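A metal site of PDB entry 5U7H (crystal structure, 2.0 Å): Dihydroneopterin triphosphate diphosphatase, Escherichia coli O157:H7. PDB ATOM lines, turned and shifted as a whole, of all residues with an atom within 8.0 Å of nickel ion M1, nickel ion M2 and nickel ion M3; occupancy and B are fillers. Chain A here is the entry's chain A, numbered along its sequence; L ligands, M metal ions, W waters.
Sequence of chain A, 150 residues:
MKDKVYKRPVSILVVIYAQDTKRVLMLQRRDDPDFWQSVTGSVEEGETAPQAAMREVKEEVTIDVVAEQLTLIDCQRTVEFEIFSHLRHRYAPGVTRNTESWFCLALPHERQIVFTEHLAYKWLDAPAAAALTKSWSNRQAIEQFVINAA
NH1 of Arg 55 touches nickel ion M3, at 3.96 Å.
Within 4 Å of nickel ion M3: Arg 55 and Glu 56.
Nickel ion M3 is bound by O4 of the ligand (2.0 Å), water W5 (2.0 Å), water W2 (2.0 Å), OE2 of Glu 56 (2.0 Å), water W4 (2.2 Å) and water W6 (2.2 Å).
Nickel ion M3 has six donor atoms within binding distance.
Nickel ion M1 is bound by O of Thr 40 (2.0 Å), water W1 (2.0 Å), O3 of the ligand (2.0 Å), OE2 of Glu 60 (2.0 Å), water W7 (2.0 Å) and OE1 of Glu 117 (2.1 Å).
Residues that only touch nickel ion M1: Gly 41.
Five residues have an atom within 4 Å of nickel ion M1: Thr 40, Gly 41, Glu 56, Glu 60 and Glu 117.
The nearest printed residue that does not touch nickel ion M1 is Arg 29 (4.3 Å).
Of the 24 residues printed, 4 come within 4 Å of nickel ion M2.
The nearest printed residue that does not touch nickel ion M2 is Glu 59 (4.1 Å).
OE2 of Glu 60 is bound to nickel ion M2, at 2.0 Å.
Nickel ion M2 is bound by OE1 of Glu 56.
Nickel ion M2 is bound by OE2 of Glu 117 (2.0 Å).
Nickel ion M2 is bound by water W5, at 2.1 Å.
Nickel ion M2 is bound by an oxygen (O3) of the ligand, 2.1 Å away.
Water W3 binds nickel ion M2, at 2.1 Å.
Water W1 lies within hydrogen-bond range of OG1 of Thr 40 and NH1 of Arg 29.
Water W7 lies within hydrogen-bond range of OE1 of Glu 60 (2.6 Å), N of Thr 40 (2.8 Å) and OE1 of Gln 37 (2.9 Å).
Water W2 bridges the guanidinium group of Arg 55 (2.9 Å) and the side-chain carboxylate of Glu 59 (3.0 Å).
Water W4 bridges the side-chain carboxylate (OE2) of Glu 44 (2.7 Å) and the backbone carbonyl oxygen (O) of Ser 42 (2.8 Å).
NH1 of Arg 55 is in salt-bridge range of OE2 of Glu 59, at 3.2 Å.
The guanidinium group (NH2) of Arg 55 sits at hydrogen-bond distance from the backbone carbonyl oxygen (O) of Ser 42 (3.2 Å).
The side-chain carboxylate (OE2) of Glu 56 sits close to the guanidinium group (NH1) of Arg 55 (2.7 Å).
The backbone carbonyl oxygen (O) of Gly 41 sits at hydrogen-bond distance from the backbone NH (N) of Ile 12.
The side-chain carboxylate of Glu 47 is in salt-bridge range of the guanidinium group of Arg 55 (2.6 Å).
OG1 of Thr 40 lies within hydrogen-bond range of NE2 of Gln 37, 3.2 Å away.
OE1 of Glu 117 sits close to NH1 of Arg 29 (3.6 Å).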
ATOM      1  N   LYS A   7      -3.234 -40.659  29.435  1.00  0.00           N
ATOM      2  CA  LYS A   7      -2.327 -39.564  29.757  1.00  0.00           C
ATOM      3  C   LYS A   7      -1.108 -40.111  30.475  1.00  0.00           C
ATOM      4  O   LYS A   7      -1.166 -41.128  31.158  1.00  0.00           O
ATOM      5  CB  LYS A   7      -3.009 -38.515  30.630  1.00  0.00           C
ATOM      6  CG  LYS A   7      -4.049 -37.667  29.915  1.00  0.00           C
ATOM      7  CD  LYS A   7      -4.699 -36.635  30.829  1.00  0.00           C
ATOM      8  CE  LYS A   7      -3.733 -35.511  31.191  1.00  0.00           C
ATOM      9  NZ  LYS A   7      -3.087 -34.932  29.960  1.00  0.00           N
ATOM     10  N   ILE A  12       4.156 -31.020  32.727  1.00  0.00           N
ATOM     11  CA  ILE A  12       4.766 -29.720  32.924  1.00  0.00           C
ATOM     12  C   ILE A  12       3.670 -28.723  33.290  1.00  0.00           C
ATOM     13  O   ILE A  12       2.484 -28.943  33.063  1.00  0.00           O
ATOM     14  CB  ILE A  12       5.536 -29.233  31.671  1.00  0.00           C
ATOM     15  CG1 ILE A  12       4.645 -29.308  30.430  1.00  0.00           C
ATOM     16  CG2 ILE A  12       6.782 -30.070  31.480  1.00  0.00           C
ATOM     17  CD1 ILE A  12       3.856 -28.053  30.129  1.00  0.00           C
ATOM     18  N   LEU A  27      -6.904 -20.354  32.476  1.00  0.00           N
ATOM     19  CA  LEU A  27      -7.666 -21.034  31.436  1.00  0.00           C
ATOM     20  C   LEU A  27      -8.626 -22.016  32.089  1.00  0.00           C
ATOM     21  O   LEU A  27      -8.267 -22.692  33.046  1.00  0.00           O
ATOM     22  CB  LEU A  27      -6.723 -21.759  30.467  1.00  0.00           C
ATOM     23  CG  LEU A  27      -5.531 -20.965  29.914  1.00  0.00           C
ATOM     24  CD1 LEU A  27      -4.490 -21.900  29.327  1.00  0.00           C
ATOM     25  CD2 LEU A  27      -6.004 -19.997  28.864  1.00  0.00           C
ATOM     26  N   ARG A  29     -10.805 -25.288  32.254  1.00  0.00           N
ATOM     27  CA  ARG A  29     -10.774 -26.629  31.679  1.00  0.00           C
ATOM     28  C   ARG A  29     -12.141 -27.037  31.136  1.00  0.00           C
ATOM     29  O   ARG A  29     -13.187 -26.557  31.573  1.00  0.00           O
ATOM     30  CB  ARG A  29     -10.298 -27.640  32.731  1.00  0.00           C
ATOM     31  CG  ARG A  29      -8.807 -27.556  33.033  1.00  0.00           C
ATOM     32  CD  ARG A  29      -8.346 -28.811  33.762  1.00  0.00           C
ATOM     33  NE  ARG A  29      -8.362 -29.983  32.896  1.00  0.00           N
ATOM     34  CZ  ARG A  29      -7.456 -30.204  31.944  1.00  0.00           C
ATOM     35  NH1 ARG A  29      -6.458 -29.348  31.746  1.00  0.00           N
ATOM     36  NH2 ARG A  29      -7.532 -31.304  31.197  1.00  0.00           N
ATOM     37  N   GLN A  37      -6.741 -22.878  35.324  1.00  0.00           N
ATOM     38  CA  GLN A  37      -5.331 -23.239  35.453  1.00  0.00           C
ATOM     39  C   GLN A  37      -4.451 -22.411  34.529  1.00  0.00           C
ATOM     40  O   GLN A  37      -4.922 -21.799  33.564  1.00  0.00           O
ATOM     41  CB  GLN A  37      -5.122 -24.704  35.112  1.00  0.00           C
ATOM     42  CG  GLN A  37      -5.678 -25.075  33.743  1.00  0.00           C
ATOM     43  CD  GLN A  37      -5.174 -26.431  33.274  1.00  0.00           C
ATOM     44  OE1 GLN A  37      -5.537 -26.907  32.188  1.00  0.00           O
ATOM     45  NE2 GLN A  37      -4.344 -27.066  34.092  1.00  0.00           N
ATOM     46  N   SER A  38      -3.160 -22.412  34.839  1.00  0.00           N
ATOM     47  CA  SER A  38      -2.129 -22.132  33.851  1.00  0.00           C
ATOM     48  C   SER A  38      -2.047 -23.284  32.846  1.00  0.00           C
ATOM     49  O   SER A  38      -2.794 -24.251  32.917  1.00  0.00           O
ATOM     50  CB  SER A  38      -0.769 -21.937  34.545  1.00  0.00           C
ATOM     51  OG  SER A  38      -0.842 -20.993  35.607  1.00  0.00           O
ATOM     52  N   VAL A  39      -1.116 -23.191  31.917  1.00  0.00           N
ATOM     53  CA  VAL A  39      -0.933 -24.263  30.934  1.00  0.00           C
ATOM     54  C   VAL A  39      -0.292 -25.468  31.621  1.00  0.00           C
ATOM     55  O   VAL A  39       0.794 -25.373  32.202  1.00  0.00           O
ATOM     56  CB  VAL A  39      -0.075 -23.786  29.757  1.00  0.00           C
ATOM     57  CG1 VAL A  39       0.355 -24.931  28.888  1.00  0.00           C
ATOM     58  CG2 VAL A  39      -0.839 -22.751  28.913  1.00  0.00           C
ATOM     59  N   THR A  40      -0.966 -26.628  31.565  1.00  0.00           N
ATOM     60  CA  THR A  40      -0.306 -27.893  31.895  1.00  0.00           C
ATOM     61  C   THR A  40      -0.422 -28.846  30.728  1.00  0.00           C
ATOM     62  O   THR A  40      -1.262 -28.676  29.846  1.00  0.00           O
ATOM     63  CB  THR A  40      -0.869 -28.551  33.169  1.00  0.00           C
ATOM     64  OG1 THR A  40      -2.172 -29.104  32.902  1.00  0.00           O
ATOM     65  CG2 THR A  40      -0.954 -27.547  34.297  1.00  0.00           C
ATOM     66  N   GLY A  41       0.459 -29.861  30.716  1.00  0.00           N
ATOM     67  CA  GLY A  41       0.417 -30.895  29.705  1.00  0.00           C
ATOM     68  C   GLY A  41       1.320 -32.092  29.995  1.00  0.00           C
ATOM     69  O   GLY A  41       2.343 -31.958  30.684  1.00  0.00           O
ATOM     70  N   SER A  42       0.939 -33.254  29.477  1.00  0.00           N
ATOM     71  CA  SER A  42       1.757 -34.447  29.671  1.00  0.00           C
ATOM     72  C   SER A  42       3.022 -34.345  28.834  1.00  0.00           C
ATOM     73  O   SER A  42       2.998 -33.884  27.696  1.00  0.00           O
ATOM     74  CB  SER A  42       0.988 -35.722  29.280  1.00  0.00           C
ATOM     75  OG  SER A  42      -0.026 -36.004  30.229  1.00  0.00           O
ATOM     76  N   VAL A  43       4.140 -34.767  29.423  1.00  0.00           N
ATOM     77  CA  VAL A  43       5.378 -34.955  28.660  1.00  0.00           C
ATOM     78  C   VAL A  43       5.279 -36.273  27.906  1.00  0.00           C
ATOM     79  O   VAL A  43       5.043 -37.325  28.514  1.00  0.00           O
ATOM     80  CB  VAL A  43       6.601 -34.930  29.581  1.00  0.00           C
ATOM     81  CG1 VAL A  43       7.867 -35.140  28.754  1.00  0.00           C
ATOM     82  CG2 VAL A  43       6.646 -33.630  30.395  1.00  0.00           C
ATOM     83  N   GLU A  44       5.475 -36.232  26.596  1.00  0.00           N
ATOM     84  CA  GLU A  44       5.364 -37.437  25.778  1.00  0.00           C
ATOM     85  C   GLU A  44       6.692 -38.171  25.685  1.00  0.00           C
ATOM     86  O   GLU A  44       7.768 -37.605  25.909  1.00  0.00           O
ATOM     87  CB  GLU A  44       4.864 -37.106  24.364  1.00  0.00           C
ATOM     88  CG  GLU A  44       3.645 -36.181  24.295  1.00  0.00           C
ATOM     89  CD  GLU A  44       2.319 -36.879  24.575  1.00  0.00           C
ATOM     90  OE1 GLU A  44       2.331 -38.057  24.997  1.00  0.00           O
ATOM     91  OE2 GLU A  44       1.259 -36.257  24.378  1.00  0.00           O
ATOM     92  N   GLU A  47      10.397 -36.900  24.478  1.00  0.00           N
ATOM     93  CA  GLU A  47      10.567 -35.457  24.560  1.00  0.00           C
ATOM     94  C   GLU A  47      10.935 -35.047  25.978  1.00  0.00           C
ATOM     95  O   GLU A  47      10.563 -35.708  26.964  1.00  0.00           O
ATOM     96  CB  GLU A  47       9.313 -34.692  24.060  1.00  0.00           C
ATOM     97  CG  GLU A  47       8.185 -34.518  25.070  1.00  0.00           C
ATOM     98  CD  GLU A  47       6.998 -33.731  24.500  1.00  0.00           C
ATOM     99  OE1 GLU A  47       7.199 -32.836  23.648  1.00  0.00           O
ATOM    100  OE2 GLU A  47       5.855 -34.034  24.916  1.00  0.00           O
ATOM    101  N   ALA A  52       8.251 -30.225  25.970  1.00  0.00           N
ATOM    102  CA  ALA A  52       6.818 -30.360  26.190  1.00  0.00           C
ATOM    103  C   ALA A  52       6.201 -29.024  26.577  1.00  0.00           C
ATOM    104  O   ALA A  52       5.080 -28.693  26.168  1.00  0.00           O
ATOM    105  CB  ALA A  52       6.538 -31.397  27.257  1.00  0.00           C
ATOM    106  N   ARG A  55       5.822 -27.048  23.411  1.00  0.00           N
ATOM    107  CA  ARG A  55       4.777 -27.627  22.558  1.00  0.00           C
ATOM    108  C   ARG A  55       3.392 -27.306  23.099  1.00  0.00           C
ATOM    109  O   ARG A  55       2.522 -26.830  22.371  1.00  0.00           O
ATOM    110  CB  ARG A  55       4.979 -29.127  22.412  1.00  0.00           C
ATOM    111  CG  ARG A  55       3.920 -29.774  21.524  1.00  0.00           C
ATOM    112  CD  ARG A  55       4.020 -31.294  21.475  1.00  0.00           C
ATOM    113  NE  ARG A  55       4.293 -31.893  22.766  1.00  0.00           N
ATOM    114  CZ  ARG A  55       3.427 -31.947  23.777  1.00  0.00           C
ATOM    115  NH1 ARG A  55       2.200 -31.465  23.648  1.00  0.00           N
ATOM    116  NH2 ARG A  55       3.806 -32.500  24.912  1.00  0.00           N
ATOM    117  N   GLU A  56       3.174 -27.551  24.410  1.00  0.00           N
ATOM    118  CA  GLU A  56       1.866 -27.289  24.988  1.00  0.00           C
ATOM    119  C   GLU A  56       1.526 -25.801  24.972  1.00  0.00           C
ATOM    120  O   GLU A  56       0.359 -25.433  24.809  1.00  0.00           O
ATOM    121  CB  GLU A  56       1.806 -27.842  26.412  1.00  0.00           C
ATOM    122  CG  GLU A  56       1.835 -29.374  26.472  1.00  0.00           C
ATOM    123  CD  GLU A  56       0.509 -30.052  26.100  1.00  0.00           C
ATOM    124  OE1 GLU A  56      -0.548 -29.393  26.102  1.00  0.00           O
ATOM    125  OE2 GLU A  56       0.539 -31.277  25.828  1.00  0.00           O
ATOM    126  N   VAL A  57       2.507 -24.916  25.141  1.00  0.00           N
ATOM    127  CA  VAL A  57       2.191 -23.494  25.042  1.00  0.00           C
ATOM    128  C   VAL A  57       1.701 -23.154  23.637  1.00  0.00           C
ATOM    129  O   VAL A  57       0.716 -22.414  23.469  1.00  0.00           O
ATOM    130  CB  VAL A  57       3.407 -22.630  25.444  1.00  0.00           C
ATOM    131  CG1 VAL A  57       3.176 -21.156  25.071  1.00  0.00           C
ATOM    132  CG2 VAL A  57       3.655 -22.760  26.960  1.00  0.00           C
ATOM    133  N   GLU A  59       0.297 -25.304  21.460  1.00  0.00           N
ATOM    134  CA  GLU A  59      -0.996 -25.965  21.275  1.00  0.00           C
ATOM    135  C   GLU A  59      -2.113 -25.230  22.011  1.00  0.00           C
ATOM    136  O   GLU A  59      -3.145 -24.907  21.428  1.00  0.00           O
ATOM    137  CB  GLU A  59      -0.924 -27.410  21.766  1.00  0.00           C
ATOM    138  CG  GLU A  59      -0.047 -28.340  20.938  1.00  0.00           C
ATOM    139  CD  GLU A  59       0.054 -29.756  21.529  1.00  0.00           C
ATOM    140  OE1 GLU A  59      -0.519 -30.004  22.629  1.00  0.00           O
ATOM    141  OE2 GLU A  59       0.714 -30.605  20.902  1.00  0.00           O
ATOM    142  N   GLU A  60      -1.916 -24.934  23.302  1.00  0.00           N
ATOM    143  CA  GLU A  60      -2.999 -24.500  24.164  1.00  0.00           C
ATOM    144  C   GLU A  60      -3.304 -23.006  24.068  1.00  0.00           C
ATOM    145  O   GLU A  60      -4.461 -22.613  24.233  1.00  0.00           O
ATOM    146  CB  GLU A  60      -2.674 -24.872  25.609  1.00  0.00           C
ATOM    147  CG  GLU A  60      -2.484 -26.367  25.774  1.00  0.00           C
ATOM    148  CD  GLU A  60      -2.753 -26.856  27.165  1.00  0.00           C
ATOM    149  OE1 GLU A  60      -3.005 -26.006  28.042  1.00  0.00           O
ATOM    150  OE2 GLU A  60      -2.726 -28.098  27.377  1.00  0.00           O
ATOM    151  N   VAL A  61      -2.312 -22.145  23.848  1.00  0.00           N
ATOM    152  CA  VAL A  61      -2.612 -20.706  23.789  1.00  0.00           C
ATOM    153  C   VAL A  61      -2.034 -20.068  22.533  1.00  0.00           C
ATOM    154  O   VAL A  61      -1.950 -18.838  22.442  1.00  0.00           O
ATOM    155  CB  VAL A  61      -2.116 -19.970  25.062  1.00  0.00           C
ATOM    156  CG1 VAL A  61      -2.820 -20.515  26.298  1.00  0.00           C
ATOM    157  CG2 VAL A  61      -0.592 -20.034  25.210  1.00  0.00           C
ATOM    158  N   ARG A  90      -8.303 -41.084  33.184  1.00  0.00           N
ATOM    159  CA  ARG A  90      -7.521 -40.860  31.982  1.00  0.00           C
ATOM    160  C   ARG A  90      -6.097 -41.432  32.076  1.00  0.00           C
ATOM    161  O   ARG A  90      -5.342 -41.326  31.100  1.00  0.00           O
ATOM    162  CB  ARG A  90      -7.472 -39.364  31.669  1.00  0.00           C
ATOM    163  CG  ARG A  90      -8.829 -38.832  31.208  1.00  0.00           C
ATOM    164  CD  ARG A  90      -9.058 -39.137  29.728  1.00  0.00           C
ATOM    165  NE  ARG A  90      -8.201 -38.294  28.890  1.00  0.00           N
ATOM    166  CZ  ARG A  90      -7.251 -38.742  28.077  1.00  0.00           C
ATOM    167  NH1 ARG A  90      -7.036 -40.049  27.965  1.00  0.00           N
ATOM    168  NH2 ARG A  90      -6.536 -37.883  27.363  1.00  0.00           N
ATOM    169  N   THR A 116      -7.437 -23.729  22.539  1.00  0.00           N
ATOM    170  CA  THR A 116      -7.990 -24.947  21.951  1.00  0.00           C
ATOM    171  C   THR A 116      -8.446 -25.996  22.958  1.00  0.00           C
ATOM    172  O   THR A 116      -9.425 -26.692  22.708  1.00  0.00           O
ATOM    173  CB  THR A 116      -6.985 -25.587  20.999  1.00  0.00           C
ATOM    174  OG1 THR A 116      -5.787 -25.939  21.725  1.00  0.00           O
ATOM    175  CG2 THR A 116      -6.617 -24.632  19.881  1.00  0.00           C
ATOM    176  N   GLU A 117      -7.766 -26.124  24.101  1.00  0.00           N
ATOM    177  CA  GLU A 117      -8.062 -27.142  25.098  1.00  0.00           C
ATOM    178  C   GLU A 117      -9.010 -26.648  26.191  1.00  0.00           C
ATOM    179  O   GLU A 117      -9.356 -27.428  27.097  1.00  0.00           O
ATOM    180  CB  GLU A 117      -6.734 -27.629  25.721  1.00  0.00           C
ATOM    181  CG  GLU A 117      -6.768 -28.858  26.672  1.00  0.00           C
ATOM    182  CD  GLU A 117      -5.361 -29.207  27.195  1.00  0.00           C
ATOM    183  OE1 GLU A 117      -5.074 -28.994  28.426  1.00  0.00           O
ATOM    184  OE2 GLU A 117      -4.554 -29.674  26.358  1.00  0.00           O
ATOM    185  N   HIS A 118      -9.472 -25.398  26.130  1.00  0.00           N
ATOM    186  CA  HIS A 118     -10.173 -24.799  27.247  1.00  0.00           C
ATOM    187  C   HIS A 118     -11.457 -24.138  26.771  1.00  0.00           C
ATOM    188  O   HIS A 118     -11.706 -24.003  25.577  1.00  0.00           O
ATOM    189  CB  HIS A 118      -9.255 -23.785  27.978  1.00  0.00           C
ATOM    190  CG  HIS A 118      -8.103 -24.435  28.695  1.00  0.00           C
ATOM    191  ND1 HIS A 118      -6.929 -24.781  28.050  1.00  0.00           N
ATOM    192  CD2 HIS A 118      -7.962 -24.841  29.980  1.00  0.00           C
ATOM    193  CE1 HIS A 118      -6.107 -25.351  28.912  1.00  0.00           C
ATOM    194  NE2 HIS A 118      -6.704 -25.394  30.100  1.00  0.00           N
HETATM  195  S1  LIG L   1      -2.689 -32.135  28.299  1.00  0.00           S
HETATM  196  O1  LIG L   1      -2.732 -32.450  29.724  1.00  0.00           O
HETATM  197  O2  LIG L   1      -3.884 -32.692  27.630  1.00  0.00           O
HETATM  198  O3  LIG L   1      -2.661 -30.661  28.094  1.00  0.00           O
HETATM  199  O4  LIG L   1      -1.500 -32.725  27.701  1.00  0.00           O
HETATM  200 NI    NI M   1      -3.062 -28.994  29.150  1.00  0.00          NI
HETATM  201 NI    NI M   2      -2.523 -29.734  26.246  1.00  0.00          NI
HETATM  202 NI    NI M   3      -0.865 -32.734  25.812  1.00  0.00          NI
HETATM  203 NI    NI M   4      -3.947 -32.847  25.608  1.00  0.00          NI
HETATM  204  O   HOH W   1      -3.627 -29.875  30.838  1.00  0.00           O
HETATM  205  O   HOH W   2      -0.370 -32.733  23.851  1.00  0.00           O
HETATM  206  O   HOH W   3      -2.432 -29.065  24.252  1.00  0.00           O
HETATM  207  O   HOH W   4       0.781 -34.121  25.965  1.00  0.00           O
HETATM  208  O   HOH W   5      -2.319 -31.479  25.186  1.00  0.00           O
HETATM  209  O   HOH W   6      -2.354 -34.327  25.383  1.00  0.00           O
HETATM  210  O   HOH W   7      -3.395 -27.308  30.251  1.00  0.00           O
